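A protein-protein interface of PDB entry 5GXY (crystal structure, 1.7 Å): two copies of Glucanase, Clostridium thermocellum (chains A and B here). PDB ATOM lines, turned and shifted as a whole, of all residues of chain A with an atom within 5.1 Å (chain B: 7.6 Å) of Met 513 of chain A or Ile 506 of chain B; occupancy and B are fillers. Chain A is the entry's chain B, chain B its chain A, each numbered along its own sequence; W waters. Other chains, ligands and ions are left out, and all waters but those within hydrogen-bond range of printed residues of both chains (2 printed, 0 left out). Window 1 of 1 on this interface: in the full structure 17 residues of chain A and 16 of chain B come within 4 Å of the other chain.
SG of Cys 509 of chain A touches CG2 of Ile 506 of chain B (3.8 Å).
Cys 509 of chain A touches Tyr 508 of chain B (O to CD1, 3.3 Å).
Gly 507 of chain B touches Glu 510 of chain A (O to O, 3.5 Å).
CA of Ser 511 of chain A touches O of Gly 507 of chain B, at 3.5 Å.
Tyr 508 of chain B touches Ser 511 of chain A (CD1 to N, 3.7 Å).
Ile 506 of chain B touches Met 513 of chain A.
Gly 507 of chain B touches Met 513 of chain A.
Asp 514 of chain A touches Ile 506 of chain B.
Val 515 of chain A touches Thr 505 of chain B.
The side-chain hydroxyl of Thr 505 of chain B is in hydrogen-bond range of the side-chain carboxylate of Asp 514 of chain A.
The side-chain sulfur (SG) of Cys 509 of chain A is disulfide-bonded to the side-chain sulfur (SG) of Cys 509 of chain B (2.1 Å).
The backbone carbonyl oxygen of Gly 507 of chain B sits at hydrogen-bond distance from the backbone NH of Gly 512 of chain A (2.9 Å).
The guanidinium group of Arg 555 of chain B is in salt-bridge range of the side-chain carboxylate of Asp 514 of chain A (3.9 Å).
O of Ile 506 of chain B sits at hydrogen-bond distance from N of Val 515 of chain A (2.8 Å).
Water W2 lies within hydrogen-bond range of the side-chain carboxylate (OD1) of Asp 514 of chain A (2.6 Å) and the side-chain carboxylate (OE1) of Glu 462 of chain B (2.6 Å).
Water W1 lies within hydrogen-bond range of the side-chain hydroxyl (OG) of Ser 511 of chain A (2.9 Å) and the side-chain amide nitrogen (NE2) of Gln 553 of chain B (2.9 Å).
Cys 509 of chain B touches its own counterpart, Cys 509 of chain A.
Positions printed for both chains: 509, 510 and 515.
Of chain B, only Ile 506 and Gly 507 come within 4 Å of Met 513 of chain A.
Of the printed residues of chain A, Gly 507 of chain B touches Glu 510, Ser 511, Gly 512 and Met 513.
Printed residues of chain A within 4 Å of Arg 555 of chain B: Asp 514.
The nearest printed residue of chain A that does not touch Cys 509 of chain B is Glu 510 of chain A (5.2 Å).
The backbone NH (N) of Gly 507 of chain B sits at hydrogen-bond distance from the backbone carbonyl oxygen (O) of Gln 553 of chain B (2.9 Å).
N of Arg 555 of chain B lies within hydrogen-bond range of O of Thr 505 of chain B (2.8 Å).
The guanidinium group (NE) of Arg 555 of chain B is in salt-bridge range of the side-chain carboxylate (OE1) of Glu 462 of chain B, at 2.9 Å.
O of Tyr 508 of chain B is in hydrogen-bond range of N of Gln 553 of chain B.
Of the 20 printed residues of chain B, 6 touch a printed residue of chain A.
Of the 12 printed residues of chain A, 7 touch a printed residue of chain B.
Printed residues of chain A that touch a printed residue of chain B: Cys 509, Glu 510, Ser 511, Gly 512, Met 513, Asp 514 and Val 515.
Among the printed residues, Asp or Glu carboxylates within 4 Å of a Lys or Arg side-chain nitrogen of the other chain: Asp 514 of chain A with Arg 555 of chain B (3.9 Å).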
ATOM      1  N   CYS A 509     -22.746 -20.384  30.220  1.00  0.00           N
ATOM      2  CA  CYS A 509     -23.189 -18.985  30.262  1.00  0.00           C
ATOM      3  C   CYS A 509     -24.623 -19.036  30.772  1.00  0.00           C
ATOM      4  O   CYS A 509     -25.509 -19.530  30.081  1.00  0.00           O
ATOM      5  CB  CYS A 509     -23.201 -18.361  28.859  1.00  0.00           C
ATOM      6  SG  CYS A 509     -21.716 -18.804  27.903  1.00  0.00           S
ATOM      7  N   GLU A 510     -24.851 -18.519  31.975  1.00  0.00           N
ATOM      8  CA  GLU A 510     -26.178 -18.589  32.584  1.00  0.00           C
ATOM      9  C   GLU A 510     -27.283 -18.010  31.695  1.00  0.00           C
ATOM     10  O   GLU A 510     -27.145 -16.909  31.156  1.00  0.00           O
ATOM     11  CB  GLU A 510     -26.152 -17.876  33.943  1.00  0.00           C
ATOM     12  CG  GLU A 510     -27.490 -17.986  34.678  1.00  0.00           C
ATOM     13  CD  GLU A 510     -27.476 -17.266  36.014  1.00  0.00           C
ATOM     14  OE1 GLU A 510     -26.389 -16.846  36.455  1.00  0.00           O
ATOM     15  OE2 GLU A 510     -28.550 -17.148  36.645  1.00  0.00           O
ATOM     16  N   SER A 511     -28.386 -18.745  31.560  1.00  0.00           N
ATOM     17  CA  SER A 511     -29.495 -18.333  30.708  1.00  0.00           C
ATOM     18  C   SER A 511     -30.045 -16.963  31.084  1.00  0.00           C
ATOM     19  O   SER A 511     -30.263 -16.693  32.265  1.00  0.00           O
ATOM     20  CB  SER A 511     -30.641 -19.343  30.820  1.00  0.00           C
ATOM     21  OG  SER A 511     -31.609 -19.071  29.820  1.00  0.00           O
ATOM     22  N   GLY A 512     -30.262 -16.119  30.081  1.00  0.00           N
ATOM     23  CA  GLY A 512     -30.863 -14.810  30.323  1.00  0.00           C
ATOM     24  C   GLY A 512     -29.902 -13.688  30.650  1.00  0.00           C
ATOM     25  O   GLY A 512     -30.327 -12.540  30.771  1.00  0.00           O
ATOM     26  N   MET A 513     -28.620 -14.001  30.808  1.00  0.00           N
ATOM     27  CA  MET A 513     -27.626 -12.977  31.110  1.00  0.00           C
ATOM     28  C   MET A 513     -26.811 -12.683  29.852  1.00  0.00           C
ATOM     29  O   MET A 513     -25.759 -13.297  29.647  1.00  0.00           O
ATOM     30  CB  MET A 513     -26.707 -13.459  32.233  1.00  0.00           C
ATOM     31  CG  MET A 513     -27.444 -13.785  33.523  1.00  0.00           C
ATOM     32  SD  MET A 513     -28.263 -12.316  34.209  1.00  0.00           S
ATOM     33  CE  MET A 513     -27.142 -10.949  33.914  1.00  0.00           C
ATOM     34  N   ASP A 514     -27.299 -11.750  29.034  1.00  0.00           N
ATOM     35  CA  ASP A 514     -26.644 -11.360  27.782  1.00  0.00           C
ATOM     36  C   ASP A 514     -25.224 -10.899  28.106  1.00  0.00           C
ATOM     37  O   ASP A 514     -25.034  -9.954  28.874  1.00  0.00           O
ATOM     38  CB  ASP A 514     -27.436 -10.246  27.085  1.00  0.00           C
ATOM     39  CG  ASP A 514     -27.017 -10.030  25.635  1.00  0.00           C
ATOM     40  OD1 ASP A 514     -26.709 -11.020  24.936  1.00  0.00           O
ATOM     41  OD2 ASP A 514     -27.059  -8.870  25.173  1.00  0.00           O
ATOM     42  N   VAL A 515     -24.232 -11.567  27.526  1.00  0.00           N
ATOM     43  CA  VAL A 515     -22.843 -11.349  27.910  1.00  0.00           C
ATOM     44  C   VAL A 515     -21.907 -11.320  26.706  1.00  0.00           C
ATOM     45  O   VAL A 515     -22.139 -12.001  25.705  1.00  0.00           O
ATOM     46  CB  VAL A 515     -22.404 -12.461  28.919  1.00  0.00           C
ATOM     47  CG1 VAL A 515     -22.375 -13.836  28.265  1.00  0.00           C
ATOM     48  CG2 VAL A 515     -21.098 -12.122  29.619  1.00  0.00           C
ATOM     49  N   TYR A 534     -21.671  -7.569  31.034  1.00  0.00           N
ATOM     50  CA  TYR A 534     -23.097  -7.860  30.950  1.00  0.00           C
ATOM     51  C   TYR A 534     -23.845  -6.688  30.317  1.00  0.00           C
ATOM     52  O   TYR A 534     -23.769  -5.553  30.796  1.00  0.00           O
ATOM     53  CB  TYR A 534     -23.646  -8.227  32.338  1.00  0.00           C
ATOM     54  CG  TYR A 534     -23.129  -9.590  32.736  1.00  0.00           C
ATOM     55  CD1 TYR A 534     -23.733 -10.736  32.234  1.00  0.00           C
ATOM     56  CD2 TYR A 534     -22.001  -9.735  33.534  1.00  0.00           C
ATOM     57  CE1 TYR A 534     -23.253 -11.994  32.546  1.00  0.00           C
ATOM     58  CE2 TYR A 534     -21.504 -11.000  33.856  1.00  0.00           C
ATOM     59  CZ  TYR A 534     -22.146 -12.117  33.363  1.00  0.00           C
ATOM     60  OH  TYR A 534     -21.705 -13.391  33.640  1.00  0.00           O
ATOM     61  N   ASP A 536     -27.121  -6.103  30.002  1.00  0.00           N
ATOM     62  CA  ASP A 536     -28.089  -5.531  30.926  1.00  0.00           C
ATOM     63  C   ASP A 536     -27.751  -6.085  32.308  1.00  0.00           C
ATOM     64  O   ASP A 536     -28.366  -7.048  32.769  1.00  0.00           O
ATOM     65  CB  ASP A 536     -29.537  -5.838  30.533  1.00  0.00           C
ATOM     66  CG  ASP A 536     -30.542  -5.138  31.428  1.00  0.00           C
ATOM     67  OD1 ASP A 536     -30.138  -4.413  32.369  1.00  0.00           O
ATOM     68  OD2 ASP A 536     -31.752  -5.327  31.198  1.00  0.00           O
ATOM     69  N   ASN A 539     -30.111  -7.168  35.425  1.00  0.00           N
ATOM     70  CA  ASN A 539     -30.602  -8.512  35.707  1.00  0.00           C
ATOM     71  C   ASN A 539     -29.752  -9.266  36.724  1.00  0.00           C
ATOM     72  O   ASN A 539     -30.153 -10.362  37.128  1.00  0.00           O
ATOM     73  CB  ASN A 539     -30.699  -9.321  34.412  1.00  0.00           C
ATOM     74  CG  ASN A 539     -31.829  -8.839  33.529  1.00  0.00           C
ATOM     75  OD1 ASN A 539     -32.893  -8.470  34.028  1.00  0.00           O
ATOM     76  ND2 ASN A 539     -31.620  -8.872  32.217  1.00  0.00           N
ATOM     77  N   ILE A 540     -28.635  -8.661  37.136  1.00  0.00           N
ATOM     78  CA  ILE A 540     -27.901  -9.128  38.315  1.00  0.00           C
ATOM     79  C   ILE A 540     -28.394  -8.288  39.497  1.00  0.00           C
ATOM     80  O   ILE A 540     -28.050  -7.112  39.613  1.00  0.00           O
ATOM     81  CB  ILE A 540     -26.375  -8.990  38.145  1.00  0.00           C
ATOM     82  CG1 ILE A 540     -25.949  -9.656  36.831  1.00  0.00           C
ATOM     83  CG2 ILE A 540     -25.656  -9.677  39.338  1.00  0.00           C
ATOM     84  CD1 ILE A 540     -24.444  -9.479  36.546  1.00  0.00           C
ATOM     85  N   ALA A 550     -24.492 -13.625  38.381  1.00  0.00           N
ATOM     86  CA  ALA A 550     -24.454 -14.193  37.036  1.00  0.00           C
ATOM     87  C   ALA A 550     -23.241 -15.111  36.971  1.00  0.00           C
ATOM     88  O   ALA A 550     -22.121 -14.690  37.253  1.00  0.00           O
ATOM     89  CB  ALA A 550     -24.323 -13.088  35.989  1.00  0.00           C
ATOM     90  N   GLU B 462     -31.710 -12.656  17.617  1.00  0.00           N
ATOM     91  CA  GLU B 462     -31.194 -13.605  18.594  1.00  0.00           C
ATOM     92  C   GLU B 462     -31.658 -15.008  18.203  1.00  0.00           C
ATOM     93  O   GLU B 462     -32.847 -15.248  17.988  1.00  0.00           O
ATOM     94  CB  GLU B 462     -31.621 -13.250  20.023  1.00  0.00           C
ATOM     95  CG  GLU B 462     -31.021 -14.192  21.073  1.00  0.00           C
ATOM     96  CD  GLU B 462     -31.336 -13.745  22.491  1.00  0.00           C
ATOM     97  OE1 GLU B 462     -30.727 -12.742  22.936  1.00  0.00           O
ATOM     98  OE2 GLU B 462     -32.190 -14.399  23.130  1.00  0.00           O
ATOM     99  N   LYS B 503     -22.484  -6.160  17.111  1.00  0.00           N
ATOM    100  CA  LYS B 503     -21.964  -6.774  18.329  1.00  0.00           C
ATOM    101  C   LYS B 503     -22.556  -8.173  18.467  1.00  0.00           C
ATOM    102  O   LYS B 503     -23.770  -8.342  18.358  1.00  0.00           O
ATOM    103  CB  LYS B 503     -22.343  -5.927  19.551  1.00  0.00           C
ATOM    104  CG  LYS B 503     -21.727  -6.416  20.859  1.00  0.00           C
ATOM    105  CD  LYS B 503     -22.146  -5.573  22.067  1.00  0.00           C
ATOM    106  CE  LYS B 503     -21.262  -4.346  22.214  1.00  0.00           C
ATOM    107  NZ  LYS B 503     -21.352  -3.763  23.583  1.00  0.00           N
ATOM    108  N   VAL B 504     -21.694  -9.155  18.714  1.00  0.00           N
ATOM    109  CA  VAL B 504     -22.145 -10.524  18.994  1.00  0.00           C
ATOM    110  C   VAL B 504     -22.069 -10.758  20.499  1.00  0.00           C
ATOM    111  O   VAL B 504     -21.050 -10.471  21.138  1.00  0.00           O
ATOM    112  CB  VAL B 504     -21.301 -11.569  18.241  1.00  0.00           C
ATOM    113  CG1 VAL B 504     -21.813 -12.987  18.493  1.00  0.00           C
ATOM    114  CG2 VAL B 504     -21.287 -11.269  16.742  1.00  0.00           C
ATOM    115  N   THR B 505     -23.179 -11.226  21.059  1.00  0.00           N
ATOM    116  CA  THR B 505     -23.249 -11.548  22.475  1.00  0.00           C
ATOM    117  C   THR B 505     -23.897 -12.925  22.643  1.00  0.00           C
ATOM    118  O   THR B 505     -24.469 -13.463  21.696  1.00  0.00           O
ATOM    119  CB  THR B 505     -24.055 -10.480  23.251  1.00  0.00           C
ATOM    120  OG1 THR B 505     -25.373 -10.350  22.704  1.00  0.00           O
ATOM    121  CG2 THR B 505     -23.369  -9.136  23.197  1.00  0.00           C
ATOM    122  N   ILE B 506     -23.808 -13.484  23.847  1.00  0.00           N
ATOM    123  CA  ILE B 506     -24.316 -14.820  24.117  1.00  0.00           C
ATOM    124  C   ILE B 506     -25.338 -14.660  25.235  1.00  0.00           C
ATOM    125  O   ILE B 506     -25.094 -13.943  26.218  1.00  0.00           O
ATOM    126  CB  ILE B 506     -23.163 -15.735  24.599  1.00  0.00           C
ATOM    127  CG1 ILE B 506     -22.183 -16.024  23.455  1.00  0.00           C
ATOM    128  CG2 ILE B 506     -23.693 -17.036  25.206  1.00  0.00           C
ATOM    129  CD1 ILE B 506     -22.830 -16.490  22.184  1.00  0.00           C
ATOM    130  N   GLY B 507     -26.478 -15.319  25.071  1.00  0.00           N
ATOM    131  CA  GLY B 507     -27.554 -15.251  26.049  1.00  0.00           C
ATOM    132  C   GLY B 507     -27.698 -16.533  26.856  1.00  0.00           C
ATOM    133  O   GLY B 507     -28.385 -16.549  27.881  1.00  0.00           O
ATOM    134  N   TYR B 508     -27.099 -17.619  26.370  1.00  0.00           N
ATOM    135  CA  TYR B 508     -27.091 -18.906  27.071  1.00  0.00           C
ATOM    136  C   TYR B 508     -26.087 -19.814  26.359  1.00  0.00           C
ATOM    137  O   TYR B 508     -26.075 -19.890  25.133  1.00  0.00           O
ATOM    138  CB  TYR B 508     -28.454 -19.603  27.064  1.00  0.00           C
ATOM    139  CG  TYR B 508     -28.427 -21.022  27.609  1.00  0.00           C
ATOM    140  CD1 TYR B 508     -28.089 -21.286  28.936  1.00  0.00           C
ATOM    141  CD2 TYR B 508     -28.717 -22.099  26.786  1.00  0.00           C
ATOM    142  CE1 TYR B 508     -28.075 -22.586  29.437  1.00  0.00           C
ATOM    143  CE2 TYR B 508     -28.697 -23.399  27.269  1.00  0.00           C
ATOM    144  CZ  TYR B 508     -28.376 -23.634  28.592  1.00  0.00           C
ATOM    145  OH  TYR B 508     -28.359 -24.927  29.038  1.00  0.00           O
ATOM    146  N   CYS B 509     -25.246 -20.488  27.129  1.00  0.00           N
ATOM    147  CA  CYS B 509     -24.420 -21.525  26.536  1.00  0.00           C
ATOM    148  C   CYS B 509     -24.423 -22.735  27.469  1.00  0.00           C
ATOM    149  O   CYS B 509     -24.166 -22.624  28.670  1.00  0.00           O
ATOM    150  CB  CYS B 509     -23.042 -20.988  26.152  1.00  0.00           C
ATOM    151  SG  CYS B 509     -21.888 -20.809  27.479  1.00  0.00           S
ATOM    152  N   GLU B 510     -24.752 -23.888  26.899  1.00  0.00           N
ATOM    153  CA  GLU B 510     -24.992 -25.080  27.703  1.00  0.00           C
ATOM    154  C   GLU B 510     -23.757 -25.505  28.486  1.00  0.00           C
ATOM    155  O   GLU B 510     -22.650 -25.498  27.948  1.00  0.00           O
ATOM    156  CB  GLU B 510     -25.459 -26.213  26.790  1.00  0.00           C
ATOM    157  CG  GLU B 510     -25.660 -27.515  27.533  1.00  0.00           C
ATOM    158  CD  GLU B 510     -26.341 -28.573  26.677  1.00  0.00           C
ATOM    159  OE1 GLU B 510     -26.755 -28.269  25.538  1.00  0.00           O
ATOM    160  OE2 GLU B 510     -26.522 -29.707  27.173  1.00  0.00           O
ATOM    161  N   VAL B 515     -16.992 -23.801  23.919  1.00  0.00           N
ATOM    162  CA  VAL B 515     -17.429 -23.219  22.655  1.00  0.00           C
ATOM    163  C   VAL B 515     -16.775 -21.862  22.379  1.00  0.00           C
ATOM    164  O   VAL B 515     -16.542 -21.068  23.291  1.00  0.00           O
ATOM    165  CB  VAL B 515     -18.977 -23.135  22.579  1.00  0.00           C
ATOM    166  CG1 VAL B 515     -19.530 -22.126  23.573  1.00  0.00           C
ATOM    167  CG2 VAL B 515     -19.454 -22.801  21.169  1.00  0.00           C
ATOM    168  N   GLU B 516     -16.460 -21.611  21.113  1.00  0.00           N
ATOM    169  CA  GLU B 516     -16.029 -20.278  20.709  1.00  0.00           C
ATOM    170  C   GLU B 516     -16.893 -19.769  19.566  1.00  0.00           C
ATOM    171  O   GLU B 516     -17.425 -20.559  18.780  1.00  0.00           O
ATOM    172  CB  GLU B 516     -14.548 -20.210  20.349  1.00  0.00           C
ATOM    173  CG  GLU B 516     -14.178 -20.993  19.131  1.00  0.00           C
ATOM    174  CD  GLU B 516     -12.775 -20.671  18.635  1.00  0.00           C
ATOM    175  OE1 GLU B 516     -12.304 -19.527  18.808  1.00  0.00           O
ATOM    176  OE2 GLU B 516     -12.145 -21.576  18.055  1.00  0.00           O
ATOM    177  N   ILE B 517     -17.038 -18.448  19.501  1.00  0.00           N
ATOM    178  CA  ILE B 517     -17.723 -17.799  18.386  1.00  0.00           C
ATOM    179  C   ILE B 517     -16.723 -16.857  17.749  1.00  0.00           C
ATOM    180  O   ILE B 517     -16.084 -16.059  18.444  1.00  0.00           O
ATOM    181  CB  ILE B 517     -18.982 -16.990  18.786  1.00  0.00           C
ATOM    182  CG1 ILE B 517     -19.955 -17.834  19.610  1.00  0.00           C
ATOM    183  CG2 ILE B 517     -19.691 -16.487  17.533  1.00  0.00           C
ATOM    184  CD1 ILE B 517     -19.543 -17.963  21.054  1.00  0.00           C
ATOM    185  N   ILE B 530     -20.559 -15.671  11.177  1.00  0.00           N
ATOM    186  CA  ILE B 530     -19.860 -16.095  12.382  1.00  0.00           C
ATOM    187  C   ILE B 530     -19.817 -17.618  12.335  1.00  0.00           C
ATOM    188  O   ILE B 530     -20.727 -18.256  11.797  1.00  0.00           O
ATOM    189  CB  ILE B 530     -20.534 -15.617  13.707  1.00  0.00           C
ATOM    190  CG1 ILE B 530     -22.000 -16.043  13.784  1.00  0.00           C
ATOM    191  CG2 ILE B 530     -20.344 -14.110  13.869  1.00  0.00           C
ATOM    192  CD1 ILE B 530     -22.619 -15.678  15.130  1.00  0.00           C
ATOM    193  N   ILE B 532     -19.539 -20.860  14.907  1.00  0.00           N
ATOM    194  CA  ILE B 532     -19.645 -21.386  16.262  1.00  0.00           C
ATOM    195  C   ILE B 532     -18.873 -22.701  16.267  1.00  0.00           C
ATOM    196  O   ILE B 532     -19.254 -23.626  15.545  1.00  0.00           O
ATOM    197  CB  ILE B 532     -21.128 -21.670  16.634  1.00  0.00           C
ATOM    198  CG1 ILE B 532     -21.948 -20.368  16.756  1.00  0.00           C
ATOM    199  CG2 ILE B 532     -21.223 -22.426  17.979  1.00  0.00           C
ATOM    200  CD1 ILE B 532     -22.137 -19.551  15.483  1.00  0.00           C
ATOM    201  N   GLU B 551     -26.749 -26.641  23.054  1.00  0.00           N
ATOM    202  CA  GLU B 551     -27.555 -25.438  22.881  1.00  0.00           C
ATOM    203  C   GLU B 551     -26.729 -24.174  23.096  1.00  0.00           C
ATOM    204  O   GLU B 551     -25.995 -24.059  24.078  1.00  0.00           O
ATOM    205  CB  GLU B 551     -28.734 -25.408  23.856  1.00  0.00           C
ATOM    206  CG  GLU B 551     -29.552 -24.119  23.734  1.00  0.00           C
ATOM    207  CD  GLU B 551     -30.866 -24.168  24.490  1.00  0.00           C
ATOM    208  OE1 GLU B 551     -31.246 -25.262  24.955  1.00  0.00           O
ATOM    209  OE2 GLU B 551     -31.527 -23.116  24.617  1.00  0.00           O
ATOM    210  N   LEU B 552     -26.859 -23.245  22.158  1.00  0.00           N
ATOM    211  CA  LEU B 552     -26.283 -21.908  22.297  1.00  0.00           C
ATOM    212  C   LEU B 552     -27.364 -20.896  21.939  1.00  0.00           C
ATOM    213  O   LEU B 552     -28.083 -21.106  20.962  1.00  0.00           O
ATOM    214  CB  LEU B 552     -25.090 -21.748  21.354  1.00  0.00           C
ATOM    215  CG  LEU B 552     -24.343 -20.404  21.335  1.00  0.00           C
ATOM    216  CD1 LEU B 552     -23.642 -20.161  22.656  1.00  0.00           C
ATOM    217  CD2 LEU B 552     -23.274 -20.344  20.235  1.00  0.00           C
ATOM    218  N   GLN B 553     -27.481 -19.795  22.688  1.00  0.00           N
ATOM    219  CA  GLN B 553     -28.308 -18.678  22.231  1.00  0.00           C
ATOM    220  C   GLN B 553     -27.362 -17.510  21.973  1.00  0.00           C
ATOM    221  O   GLN B 553     -26.583 -17.132  22.853  1.00  0.00           O
ATOM    222  CB  GLN B 553     -29.387 -18.319  23.259  1.00  0.00           C
ATOM    223  CG  GLN B 553     -30.389 -19.442  23.485  1.00  0.00           C
ATOM    224  CD  GLN B 553     -31.220 -19.243  24.742  1.00  0.00           C
ATOM    225  OE1 GLN B 553     -31.358 -18.128  25.245  1.00  0.00           O
ATOM    226  NE2 GLN B 553     -31.763 -20.334  25.262  1.00  0.00           N
ATOM    227  N   PHE B 554     -27.365 -17.011  20.741  1.00  0.00           N
ATOM    228  CA  PHE B 554     -26.460 -15.918  20.376  1.00  0.00           C
ATOM    229  C   PHE B 554     -27.237 -14.773  19.764  1.00  0.00           C
ATOM    230  O   PHE B 554     -28.263 -14.977  19.120  1.00  0.00           O
ATOM    231  CB  PHE B 554     -25.310 -16.348  19.447  1.00  0.00           C
ATOM    232  CG  PHE B 554     -25.748 -16.968  18.136  1.00  0.00           C
ATOM    233  CD1 PHE B 554     -25.975 -16.178  17.016  1.00  0.00           C
ATOM    234  CD2 PHE B 554     -25.876 -18.350  18.017  1.00  0.00           C
ATOM    235  CE1 PHE B 554     -26.343 -16.740  15.796  1.00  0.00           C
ATOM    236  CE2 PHE B 554     -26.249 -18.937  16.805  1.00  0.00           C
ATOM    237  CZ  PHE B 554     -26.478 -18.127  15.686  1.00  0.00           C
ATOM    238  N   ARG B 555     -26.738 -13.564  19.975  1.00  0.00           N
ATOM    239  CA  ARG B 555     -27.418 -12.371  19.508  1.00  0.00           C
ATOM    240  C   ARG B 555     -26.431 -11.601  18.642  1.00  0.00           C
ATOM    241  O   ARG B 555     -25.263 -11.446  19.010  1.00  0.00           O
ATOM    242  CB  ARG B 555     -27.900 -11.523  20.696  1.00  0.00           C
ATOM    243  CG  ARG B 555     -28.506 -10.185  20.278  1.00  0.00           C
ATOM    244  CD  ARG B 555     -28.914  -9.326  21.480  1.00  0.00           C
ATOM    245  NE  ARG B 555     -29.874 -10.010  22.342  1.00  0.00           N
ATOM    246  CZ  ARG B 555     -30.580  -9.409  23.297  1.00  0.00           C
ATOM    247  NH1 ARG B 555     -30.449  -8.103  23.492  1.00  0.00           N
ATOM    248  NH2 ARG B 555     -31.432 -10.111  24.035  1.00  0.00           N
ATOM    249  N   ILE B 556     -26.914 -11.125  17.495  1.00  0.00           N
ATOM    250  CA  ILE B 556     -26.130 -10.311  16.563  1.00  0.00           C
ATOM    251  C   ILE B 556     -26.914  -9.009  16.475  1.00  0.00           C
ATOM    252  O   ILE B 556     -28.075  -9.020  16.056  1.00  0.00           O
ATOM    253  CB  ILE B 556     -26.017 -10.967  15.174  1.00  0.00           C
ATOM    254  CG1 ILE B 556     -25.374 -12.352  15.322  1.00  0.00           C
ATOM    255  CG2 ILE B 556     -25.149 -10.114  14.253  1.00  0.00           C
ATOM    256  CD1 ILE B 556     -25.622 -13.277  14.142  1.00  0.00           C
HETATM  257  O   HOH W   1     -32.751 -20.922  27.918  1.00  0.00           O
HETATM  258  O   HOH W   2     -28.768 -12.526  24.670  1.00  0.00           O
